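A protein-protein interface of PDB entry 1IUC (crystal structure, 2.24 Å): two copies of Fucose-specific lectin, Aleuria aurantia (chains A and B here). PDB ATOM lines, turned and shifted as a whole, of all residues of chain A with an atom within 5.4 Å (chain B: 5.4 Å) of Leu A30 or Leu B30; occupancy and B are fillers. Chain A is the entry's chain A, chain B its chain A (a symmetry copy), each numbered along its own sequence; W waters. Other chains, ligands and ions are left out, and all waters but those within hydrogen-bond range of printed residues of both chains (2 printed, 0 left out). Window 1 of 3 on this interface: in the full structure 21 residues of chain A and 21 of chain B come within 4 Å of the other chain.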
ATOM      1  N   THR A   2      11.624  -2.613  29.528  1.00  0.00           N
ATOM      2  CA  THR A   2      11.362  -3.732  30.425  1.00  0.00           C
ATOM      3  C   THR A   2      12.651  -4.502  30.670  1.00  0.00           C
ATOM      4  O   THR A   2      13.715  -4.120  30.185  1.00  0.00           O
ATOM      5  CB  THR A   2      10.343  -4.711  29.801  1.00  0.00           C
ATOM      6  OG1 THR A   2      10.976  -5.432  28.734  1.00  0.00           O
ATOM      7  CG2 THR A   2       9.145  -3.957  29.233  1.00  0.00           C
ATOM      8  N   GLU A   3      12.547  -5.614  31.392  1.00  0.00           N
ATOM      9  CA  GLU A   3      13.723  -6.421  31.684  1.00  0.00           C
ATOM     10  C   GLU A   3      13.787  -7.669  30.817  1.00  0.00           C
ATOM     11  O   GLU A   3      14.595  -8.564  31.061  1.00  0.00           O
ATOM     12  CB  GLU A   3      13.731  -6.781  33.168  1.00  0.00           C
ATOM     13  CG  GLU A   3      13.716  -5.542  34.036  1.00  0.00           C
ATOM     14  CD  GLU A   3      13.701  -5.848  35.517  1.00  0.00           C
ATOM     15  OE1 GLU A   3      12.794  -6.575  35.984  1.00  0.00           O
ATOM     16  OE2 GLU A   3      14.599  -5.343  36.218  1.00  0.00           O
ATOM     17  N   PHE A   4      12.934  -7.707  29.795  1.00  0.00           N
ATOM     18  CA  PHE A   4      12.860  -8.824  28.844  1.00  0.00           C
ATOM     19  C   PHE A   4      14.069  -8.689  27.926  1.00  0.00           C
ATOM     20  O   PHE A   4      14.274  -7.636  27.312  1.00  0.00           O
ATOM     21  CB  PHE A   4      11.556  -8.708  28.040  1.00  0.00           C
ATOM     22  CG  PHE A   4      11.205  -9.928  27.199  1.00  0.00           C
ATOM     23  CD1 PHE A   4      11.902 -11.122  27.315  1.00  0.00           C
ATOM     24  CD2 PHE A   4      10.129  -9.871  26.307  1.00  0.00           C
ATOM     25  CE1 PHE A   4      11.541 -12.243  26.562  1.00  0.00           C
ATOM     26  CE2 PHE A   4       9.758 -10.990  25.548  1.00  0.00           C
ATOM     27  CZ  PHE A   4      10.469 -12.175  25.681  1.00  0.00           C
ATOM     28  N   LEU A   5      14.879  -9.739  27.848  1.00  0.00           N
ATOM     29  CA  LEU A   5      16.062  -9.728  27.001  1.00  0.00           C
ATOM     30  C   LEU A   5      15.669  -9.838  25.528  1.00  0.00           C
ATOM     31  O   LEU A   5      14.928 -10.753  25.135  1.00  0.00           O
ATOM     32  CB  LEU A   5      16.981 -10.906  27.361  1.00  0.00           C
ATOM     33  CG  LEU A   5      18.267 -11.103  26.543  1.00  0.00           C
ATOM     34  CD1 LEU A   5      19.288 -10.028  26.912  1.00  0.00           C
ATOM     35  CD2 LEU A   5      18.853 -12.485  26.816  1.00  0.00           C
ATOM     36  N   TYR A   6      16.166  -8.904  24.714  1.00  0.00           N
ATOM     37  CA  TYR A   6      15.894  -8.911  23.282  1.00  0.00           C
ATOM     38  C   TYR A   6      16.531 -10.155  22.642  1.00  0.00           C
ATOM     39  O   TYR A   6      17.726 -10.420  22.802  1.00  0.00           O
ATOM     40  CB  TYR A   6      16.444  -7.636  22.635  1.00  0.00           C
ATOM     41  CG  TYR A   6      16.286  -7.610  21.131  1.00  0.00           C
ATOM     42  CD1 TYR A   6      15.036  -7.798  20.541  1.00  0.00           C
ATOM     43  CD2 TYR A   6      17.386  -7.400  20.300  1.00  0.00           C
ATOM     44  CE1 TYR A   6      14.887  -7.775  19.155  1.00  0.00           C
ATOM     45  CE2 TYR A   6      17.247  -7.372  18.919  1.00  0.00           C
ATOM     46  CZ  TYR A   6      15.995  -7.560  18.354  1.00  0.00           C
ATOM     47  OH  TYR A   6      15.855  -7.540  16.990  1.00  0.00           O
ATOM     48  N   GLN A  28      13.909 -15.132  29.428  1.00  0.00           N
ATOM     49  CA  GLN A  28      15.136 -14.693  30.088  1.00  0.00           C
ATOM     50  C   GLN A  28      15.197 -13.171  30.279  1.00  0.00           C
ATOM     51  O   GLN A  28      14.735 -12.397  29.426  1.00  0.00           O
ATOM     52  CB  GLN A  28      16.322 -15.189  29.263  1.00  0.00           C
ATOM     53  CG  GLN A  28      17.673 -15.075  29.912  1.00  0.00           C
ATOM     54  CD  GLN A  28      18.704 -15.951  29.225  1.00  0.00           C
ATOM     55  OE1 GLN A  28      18.806 -15.966  27.999  1.00  0.00           O
ATOM     56  NE2 GLN A  28      19.482 -16.685  30.020  1.00  0.00           N
ATOM     57  N   ASP A  29      15.747 -12.732  31.408  1.00  0.00           N
ATOM     58  CA  ASP A  29      15.866 -11.300  31.651  1.00  0.00           C
ATOM     59  C   ASP A  29      17.262 -10.807  31.290  1.00  0.00           C
ATOM     60  O   ASP A  29      18.122 -11.593  30.886  1.00  0.00           O
ATOM     61  CB  ASP A  29      15.509 -10.944  33.108  1.00  0.00           C
ATOM     62  CG  ASP A  29      16.467 -11.540  34.138  1.00  0.00           C
ATOM     63  OD1 ASP A  29      17.630 -11.845  33.808  1.00  0.00           O
ATOM     64  OD2 ASP A  29      16.045 -11.672  35.311  1.00  0.00           O
ATOM     65  N   LEU A  30      17.481  -9.503  31.411  1.00  0.00           N
ATOM     66  CA  LEU A  30      18.773  -8.897  31.076  1.00  0.00           C
ATOM     67  C   LEU A  30      19.964  -9.506  31.830  1.00  0.00           C
ATOM     68  O   LEU A  30      21.111  -9.386  31.388  1.00  0.00           O
ATOM     69  CB  LEU A  30      18.709  -7.390  31.336  1.00  0.00           C
ATOM     70  CG  LEU A  30      17.621  -6.621  30.576  1.00  0.00           C
ATOM     71  CD1 LEU A  30      17.653  -5.165  30.980  1.00  0.00           C
ATOM     72  CD2 LEU A  30      17.844  -6.735  29.070  1.00  0.00           C
ATOM     73  N   ASN A  31      19.699 -10.163  32.959  1.00  0.00           N
ATOM     74  CA  ASN A  31      20.770 -10.778  33.747  1.00  0.00           C
ATOM     75  C   ASN A  31      21.031 -12.246  33.469  1.00  0.00           C
ATOM     76  O   ASN A  31      21.913 -12.838  34.094  1.00  0.00           O
ATOM     77  CB  ASN A  31      20.498 -10.622  35.236  1.00  0.00           C
ATOM     78  CG  ASN A  31      20.588  -9.189  35.680  1.00  0.00           C
ATOM     79  OD1 ASN A  31      19.733  -8.708  36.419  1.00  0.00           O
ATOM     80  ND2 ASN A  31      21.626  -8.490  35.226  1.00  0.00           N
ATOM     81  N   GLY A  32      20.281 -12.842  32.546  1.00  0.00           N
ATOM     82  CA  GLY A  32      20.498 -14.250  32.252  1.00  0.00           C
ATOM     83  C   GLY A  32      19.596 -15.155  33.079  1.00  0.00           C
ATOM     84  O   GLY A  32      19.634 -16.378  32.936  1.00  0.00           O
ATOM     85  N   LEU A  59      23.402 -16.339  28.617  1.00  0.00           N
ATOM     86  CA  LEU A  59      22.576 -15.341  27.950  1.00  0.00           C
ATOM     87  C   LEU A  59      22.218 -15.877  26.562  1.00  0.00           C
ATOM     88  O   LEU A  59      23.051 -16.494  25.890  1.00  0.00           O
ATOM     89  CB  LEU A  59      23.330 -14.003  27.849  1.00  0.00           C
ATOM     90  CG  LEU A  59      23.406 -13.224  29.171  1.00  0.00           C
ATOM     91  CD1 LEU A  59      24.508 -12.178  29.097  1.00  0.00           C
ATOM     92  CD2 LEU A  59      22.074 -12.560  29.447  1.00  0.00           C
ATOM     93  N   PHE A  60      20.980 -15.642  26.147  1.00  0.00           N
ATOM     94  CA  PHE A  60      20.465 -16.110  24.855  1.00  0.00           C
ATOM     95  C   PHE A  60      20.379 -17.640  24.779  1.00  0.00           C
ATOM     96  O   PHE A  60      20.416 -18.245  23.707  1.00  0.00           O
ATOM     97  CB  PHE A  60      21.308 -15.552  23.710  1.00  0.00           C
ATOM     98  CG  PHE A  60      21.484 -14.060  23.777  1.00  0.00           C
ATOM     99  CD1 PHE A  60      22.664 -13.502  24.279  1.00  0.00           C
ATOM    100  CD2 PHE A  60      20.449 -13.212  23.405  1.00  0.00           C
ATOM    101  CE1 PHE A  60      22.804 -12.117  24.410  1.00  0.00           C
ATOM    102  CE2 PHE A  60      20.579 -11.830  23.532  1.00  0.00           C
ATOM    103  CZ  PHE A  60      21.761 -11.283  24.038  1.00  0.00           C
ATOM    104  N   THR B   2      25.798 -10.378  21.100  1.00  0.00           N
ATOM    105  CA  THR B   2      26.809  -9.513  21.697  1.00  0.00           C
ATOM    106  C   THR B   2      26.321  -9.017  23.049  1.00  0.00           C
ATOM    107  O   THR B   2      25.243  -9.394  23.508  1.00  0.00           O
ATOM    108  CB  THR B   2      27.070  -8.277  20.810  1.00  0.00           C
ATOM    109  OG1 THR B   2      25.947  -7.388  20.898  1.00  0.00           O
ATOM    110  CG2 THR B   2      27.253  -8.685  19.352  1.00  0.00           C
ATOM    111  N   GLU B   3      27.097  -8.133  23.671  1.00  0.00           N
ATOM    112  CA  GLU B   3      26.719  -7.599  24.971  1.00  0.00           C
ATOM    113  C   GLU B   3      26.169  -6.185  24.866  1.00  0.00           C
ATOM    114  O   GLU B   3      25.987  -5.503  25.874  1.00  0.00           O
ATOM    115  CB  GLU B   3      27.925  -7.652  25.907  1.00  0.00           C
ATOM    116  CG  GLU B   3      28.447  -9.064  26.052  1.00  0.00           C
ATOM    117  CD  GLU B   3      29.657  -9.164  26.955  1.00  0.00           C
ATOM    118  OE1 GLU B   3      30.671  -8.474  26.702  1.00  0.00           O
ATOM    119  OE2 GLU B   3      29.592  -9.954  27.918  1.00  0.00           O
ATOM    120  N   PHE B   4      25.891  -5.762  23.633  1.00  0.00           N
ATOM    121  CA  PHE B   4      25.342  -4.432  23.339  1.00  0.00           C
ATOM    122  C   PHE B   4      23.870  -4.478  23.734  1.00  0.00           C
ATOM    123  O   PHE B   4      23.124  -5.347  23.268  1.00  0.00           O
ATOM    124  CB  PHE B   4      25.489  -4.154  21.835  1.00  0.00           C
ATOM    125  CG  PHE B   4      25.207  -2.719  21.412  1.00  0.00           C
ATOM    126  CD1 PHE B   4      25.033  -1.703  22.342  1.00  0.00           C
ATOM    127  CD2 PHE B   4      25.155  -2.391  20.054  1.00  0.00           C
ATOM    128  CE1 PHE B   4      24.814  -0.384  21.935  1.00  0.00           C
ATOM    129  CE2 PHE B   4      24.936  -1.072  19.635  1.00  0.00           C
ATOM    130  CZ  PHE B   4      24.766  -0.071  20.582  1.00  0.00           C
ATOM    131  N   LEU B   5      23.457  -3.563  24.604  1.00  0.00           N
ATOM    132  CA  LEU B   5      22.074  -3.505  25.051  1.00  0.00           C
ATOM    133  C   LEU B   5      21.174  -2.955  23.944  1.00  0.00           C
ATOM    134  O   LEU B   5      21.439  -1.878  23.387  1.00  0.00           O
ATOM    135  CB  LEU B   5      21.954  -2.600  26.286  1.00  0.00           C
ATOM    136  CG  LEU B   5      20.559  -2.365  26.886  1.00  0.00           C
ATOM    137  CD1 LEU B   5      20.084  -3.627  27.606  1.00  0.00           C
ATOM    138  CD2 LEU B   5      20.601  -1.198  27.867  1.00  0.00           C
ATOM    139  N   TYR B   6      20.110  -3.697  23.626  1.00  0.00           N
ATOM    140  CA  TYR B   6      19.155  -3.272  22.610  1.00  0.00           C
ATOM    141  C   TYR B   6      18.433  -1.998  23.081  1.00  0.00           C
ATOM    142  O   TYR B   6      17.868  -1.948  24.177  1.00  0.00           O
ATOM    143  CB  TYR B   6      18.144  -4.389  22.337  1.00  0.00           C
ATOM    144  CG  TYR B   6      17.059  -3.992  21.362  1.00  0.00           C
ATOM    145  CD1 TYR B   6      17.382  -3.488  20.101  1.00  0.00           C
ATOM    146  CD2 TYR B   6      15.712  -4.118  21.699  1.00  0.00           C
ATOM    147  CE1 TYR B   6      16.384  -3.121  19.199  1.00  0.00           C
ATOM    148  CE2 TYR B   6      14.711  -3.757  20.806  1.00  0.00           C
ATOM    149  CZ  TYR B   6      15.056  -3.260  19.559  1.00  0.00           C
ATOM    150  OH  TYR B   6      14.070  -2.897  18.677  1.00  0.00           O
ATOM    151  N   GLN B  28      26.004   1.293  26.171  1.00  0.00           N
ATOM    152  CA  GLN B  28      25.717   0.534  27.385  1.00  0.00           C
ATOM    153  C   GLN B  28      25.626  -0.978  27.134  1.00  0.00           C
ATOM    154  O   GLN B  28      25.135  -1.427  26.087  1.00  0.00           O
ATOM    155  CB  GLN B  28      24.416   1.069  27.981  1.00  0.00           C
ATOM    156  CG  GLN B  28      24.087   0.606  29.374  1.00  0.00           C
ATOM    157  CD  GLN B  28      23.041   1.488  30.028  1.00  0.00           C
ATOM    158  OE1 GLN B  28      22.021   1.816  29.423  1.00  0.00           O
ATOM    159  NE2 GLN B  28      23.288   1.872  31.280  1.00  0.00           N
ATOM    160  N   ASP B  29      26.117  -1.772  28.082  1.00  0.00           N
ATOM    161  CA  ASP B  29      26.043  -3.219  27.931  1.00  0.00           C
ATOM    162  C   ASP B  29      24.846  -3.780  28.689  1.00  0.00           C
ATOM    163  O   ASP B  29      24.112  -3.037  29.345  1.00  0.00           O
ATOM    164  CB  ASP B  29      27.353  -3.900  28.375  1.00  0.00           C
ATOM    165  CG  ASP B  29      27.657  -3.733  29.863  1.00  0.00           C
ATOM    166  OD1 ASP B  29      26.732  -3.510  30.669  1.00  0.00           O
ATOM    167  OD2 ASP B  29      28.849  -3.864  30.228  1.00  0.00           O
ATOM    168  N   LEU B  30      24.634  -5.086  28.581  1.00  0.00           N
ATOM    169  CA  LEU B  30      23.505  -5.748  29.242  1.00  0.00           C
ATOM    170  C   LEU B  30      23.453  -5.527  30.761  1.00  0.00           C
ATOM    171  O   LEU B  30      22.393  -5.677  31.378  1.00  0.00           O
ATOM    172  CB  LEU B  30      23.546  -7.247  28.937  1.00  0.00           C
ATOM    173  CG  LEU B  30      23.510  -7.633  27.452  1.00  0.00           C
ATOM    174  CD1 LEU B  30      23.612  -9.135  27.316  1.00  0.00           C
ATOM    175  CD2 LEU B  30      22.211  -7.152  26.811  1.00  0.00           C
ATOM    176  N   ASN B  31      24.586  -5.165  31.364  1.00  0.00           N
ATOM    177  CA  ASN B  31      24.633  -4.931  32.809  1.00  0.00           C
ATOM    178  C   ASN B  31      24.454  -3.491  33.248  1.00  0.00           C
ATOM    179  O   ASN B  31      24.486  -3.211  34.448  1.00  0.00           O
ATOM    180  CB  ASN B  31      25.944  -5.441  33.391  1.00  0.00           C
ATOM    181  CG  ASN B  31      26.045  -6.939  33.329  1.00  0.00           C
ATOM    182  OD1 ASN B  31      27.079  -7.481  32.947  1.00  0.00           O
ATOM    183  ND2 ASN B  31      24.966  -7.624  33.700  1.00  0.00           N
ATOM    184  N   GLY B  32      24.266  -2.576  32.301  1.00  0.00           N
ATOM    185  CA  GLY B  32      24.093  -1.182  32.681  1.00  0.00           C
ATOM    186  C   GLY B  32      25.410  -0.418  32.681  1.00  0.00           C
ATOM    187  O   GLY B  32      25.438   0.781  32.957  1.00  0.00           O
ATOM    188  N   LEU B  59      19.762   1.393  33.468  1.00  0.00           N
ATOM    189  CA  LEU B  59      19.608   0.728  32.180  1.00  0.00           C
ATOM    190  C   LEU B  59      18.811   1.658  31.263  1.00  0.00           C
ATOM    191  O   LEU B  59      17.861   2.314  31.702  1.00  0.00           O
ATOM    192  CB  LEU B  59      18.892  -0.622  32.357  1.00  0.00           C
ATOM    193  CG  LEU B  59      19.776  -1.729  32.952  1.00  0.00           C
ATOM    194  CD1 LEU B  59      18.909  -2.854  33.494  1.00  0.00           C
ATOM    195  CD2 LEU B  59      20.713  -2.258  31.887  1.00  0.00           C
ATOM    196  N   PHE B  60      19.207   1.710  29.997  1.00  0.00           N
ATOM    197  CA  PHE B  60      18.571   2.570  28.993  1.00  0.00           C
ATOM    198  C   PHE B  60      18.767   4.062  29.291  1.00  0.00           C
ATOM    199  O   PHE B  60      17.987   4.920  28.878  1.00  0.00           O
ATOM    200  CB  PHE B  60      17.088   2.230  28.860  1.00  0.00           C
ATOM    201  CG  PHE B  60      16.834   0.764  28.638  1.00  0.00           C
ATOM    202  CD1 PHE B  60      16.435  -0.059  29.695  1.00  0.00           C
ATOM    203  CD2 PHE B  60      17.058   0.192  27.393  1.00  0.00           C
ATOM    204  CE1 PHE B  60      16.268  -1.436  29.509  1.00  0.00           C
ATOM    205  CE2 PHE B  60      16.894  -1.178  27.197  1.00  0.00           C
ATOM    206  CZ  PHE B  60      16.499  -1.993  28.260  1.00  0.00           C
HETATM  207  O   HOH W   1      21.287  -5.993  33.787  1.00  0.00           O
HETATM  208  O   HOH W   2      23.712  -9.578  31.960  1.00  0.00           O
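Phe B60 touches Thr A2. Tyr A6 touches Tyr B6 (CG to CD2, 3.6 Å). O of Leu A30 touches O of Leu B30, 3.9 Å away. Leu B59 touches Leu A30 (CD1 to CD1, 3.6 Å). Asn A31 touches Asn B31 (ND2 to ND2, 3.8 Å). Leu B30 touches Leu A59 (CD1 to CD1, 3.6 Å). CE1 of Phe A60 touches O of Thr B2 (3.8 Å).
Water W1 bridges the backbone carbonyl oxygen of Leu B30 (2.7 Å) and the side-chain amide nitrogen of Asn A31 (2.9 Å). Water W2 lies within hydrogen-bond range of O of Leu A30 and ND2 of Asn B31.
Of the printed residues of chain B, Thr A2 touches Phe B60. Of the printed residues of chain B, Tyr A6 touches Tyr B6 (3.6 Å). Of the printed residues of chain B, Asn A31 touches Asn B31. Phe B4 touches none of the printed residues of chain A. Printed residues of chain A within 4 Å of Tyr B6: Tyr A6. Leu B30 touches just these residues of chain A: Leu A30 (3.9 Å) and Leu A59 (3.6 Å). Gly B32 touches none of the printed residues of chain A. Of the printed residues of chain A, Leu B59 touches Leu A30 (3.6 Å). The nearest residue of chain B that does not touch Leu A30 is Leu B5 (4.1 Å).
The side-chain hydroxyl (OG1) of Thr A2 is in hydrogen-bond range of the backbone NH (N) of Phe A4 (3.2 Å). The backbone carbonyl oxygen (O) of Glu A3 is in hydrogen-bond range of the backbone NH (N) of Leu A30, at 3.1 Å. The side-chain amide oxygen (OE1) of Gln A28 is in hydrogen-bond range of the backbone NH (N) of Phe A60 (2.9 Å). The side-chain carboxylate (OD1) of Asp A29 is in hydrogen-bond range of the backbone NH (N) of Asn A31 (2.8 Å). N of Leu B30 is in hydrogen-bond range of O of Glu B3, 3.1 Å away. OE1 of Gln B28 is in hydrogen-bond range of N of Phe B60, 2.9 Å away.
Thr A2 touches Phe B60, and with the chains exchanged Phe A60 touches Thr B2. Tyr A6 touches its own counterpart, Tyr B6. Leu B30 touches its own counterpart, Leu A30. Leu A30 touches Leu B59, and with the chains exchanged Leu A59 touches Leu B30. Positions printed for both chains: 2, 3, 4, 5, 6, 28, 29, 30, 31, 32, 59 and 60.
Of the 12 printed residues of chain A, 6 touch a printed residue of chain B. Hydrophobic or aromatic side chains of chain A within 4 Å of the printed part of chain B: Tyr A6, Leu A30, Leu A59 and Phe A60. Among the printed residues, 7 pairs touch across the chains.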
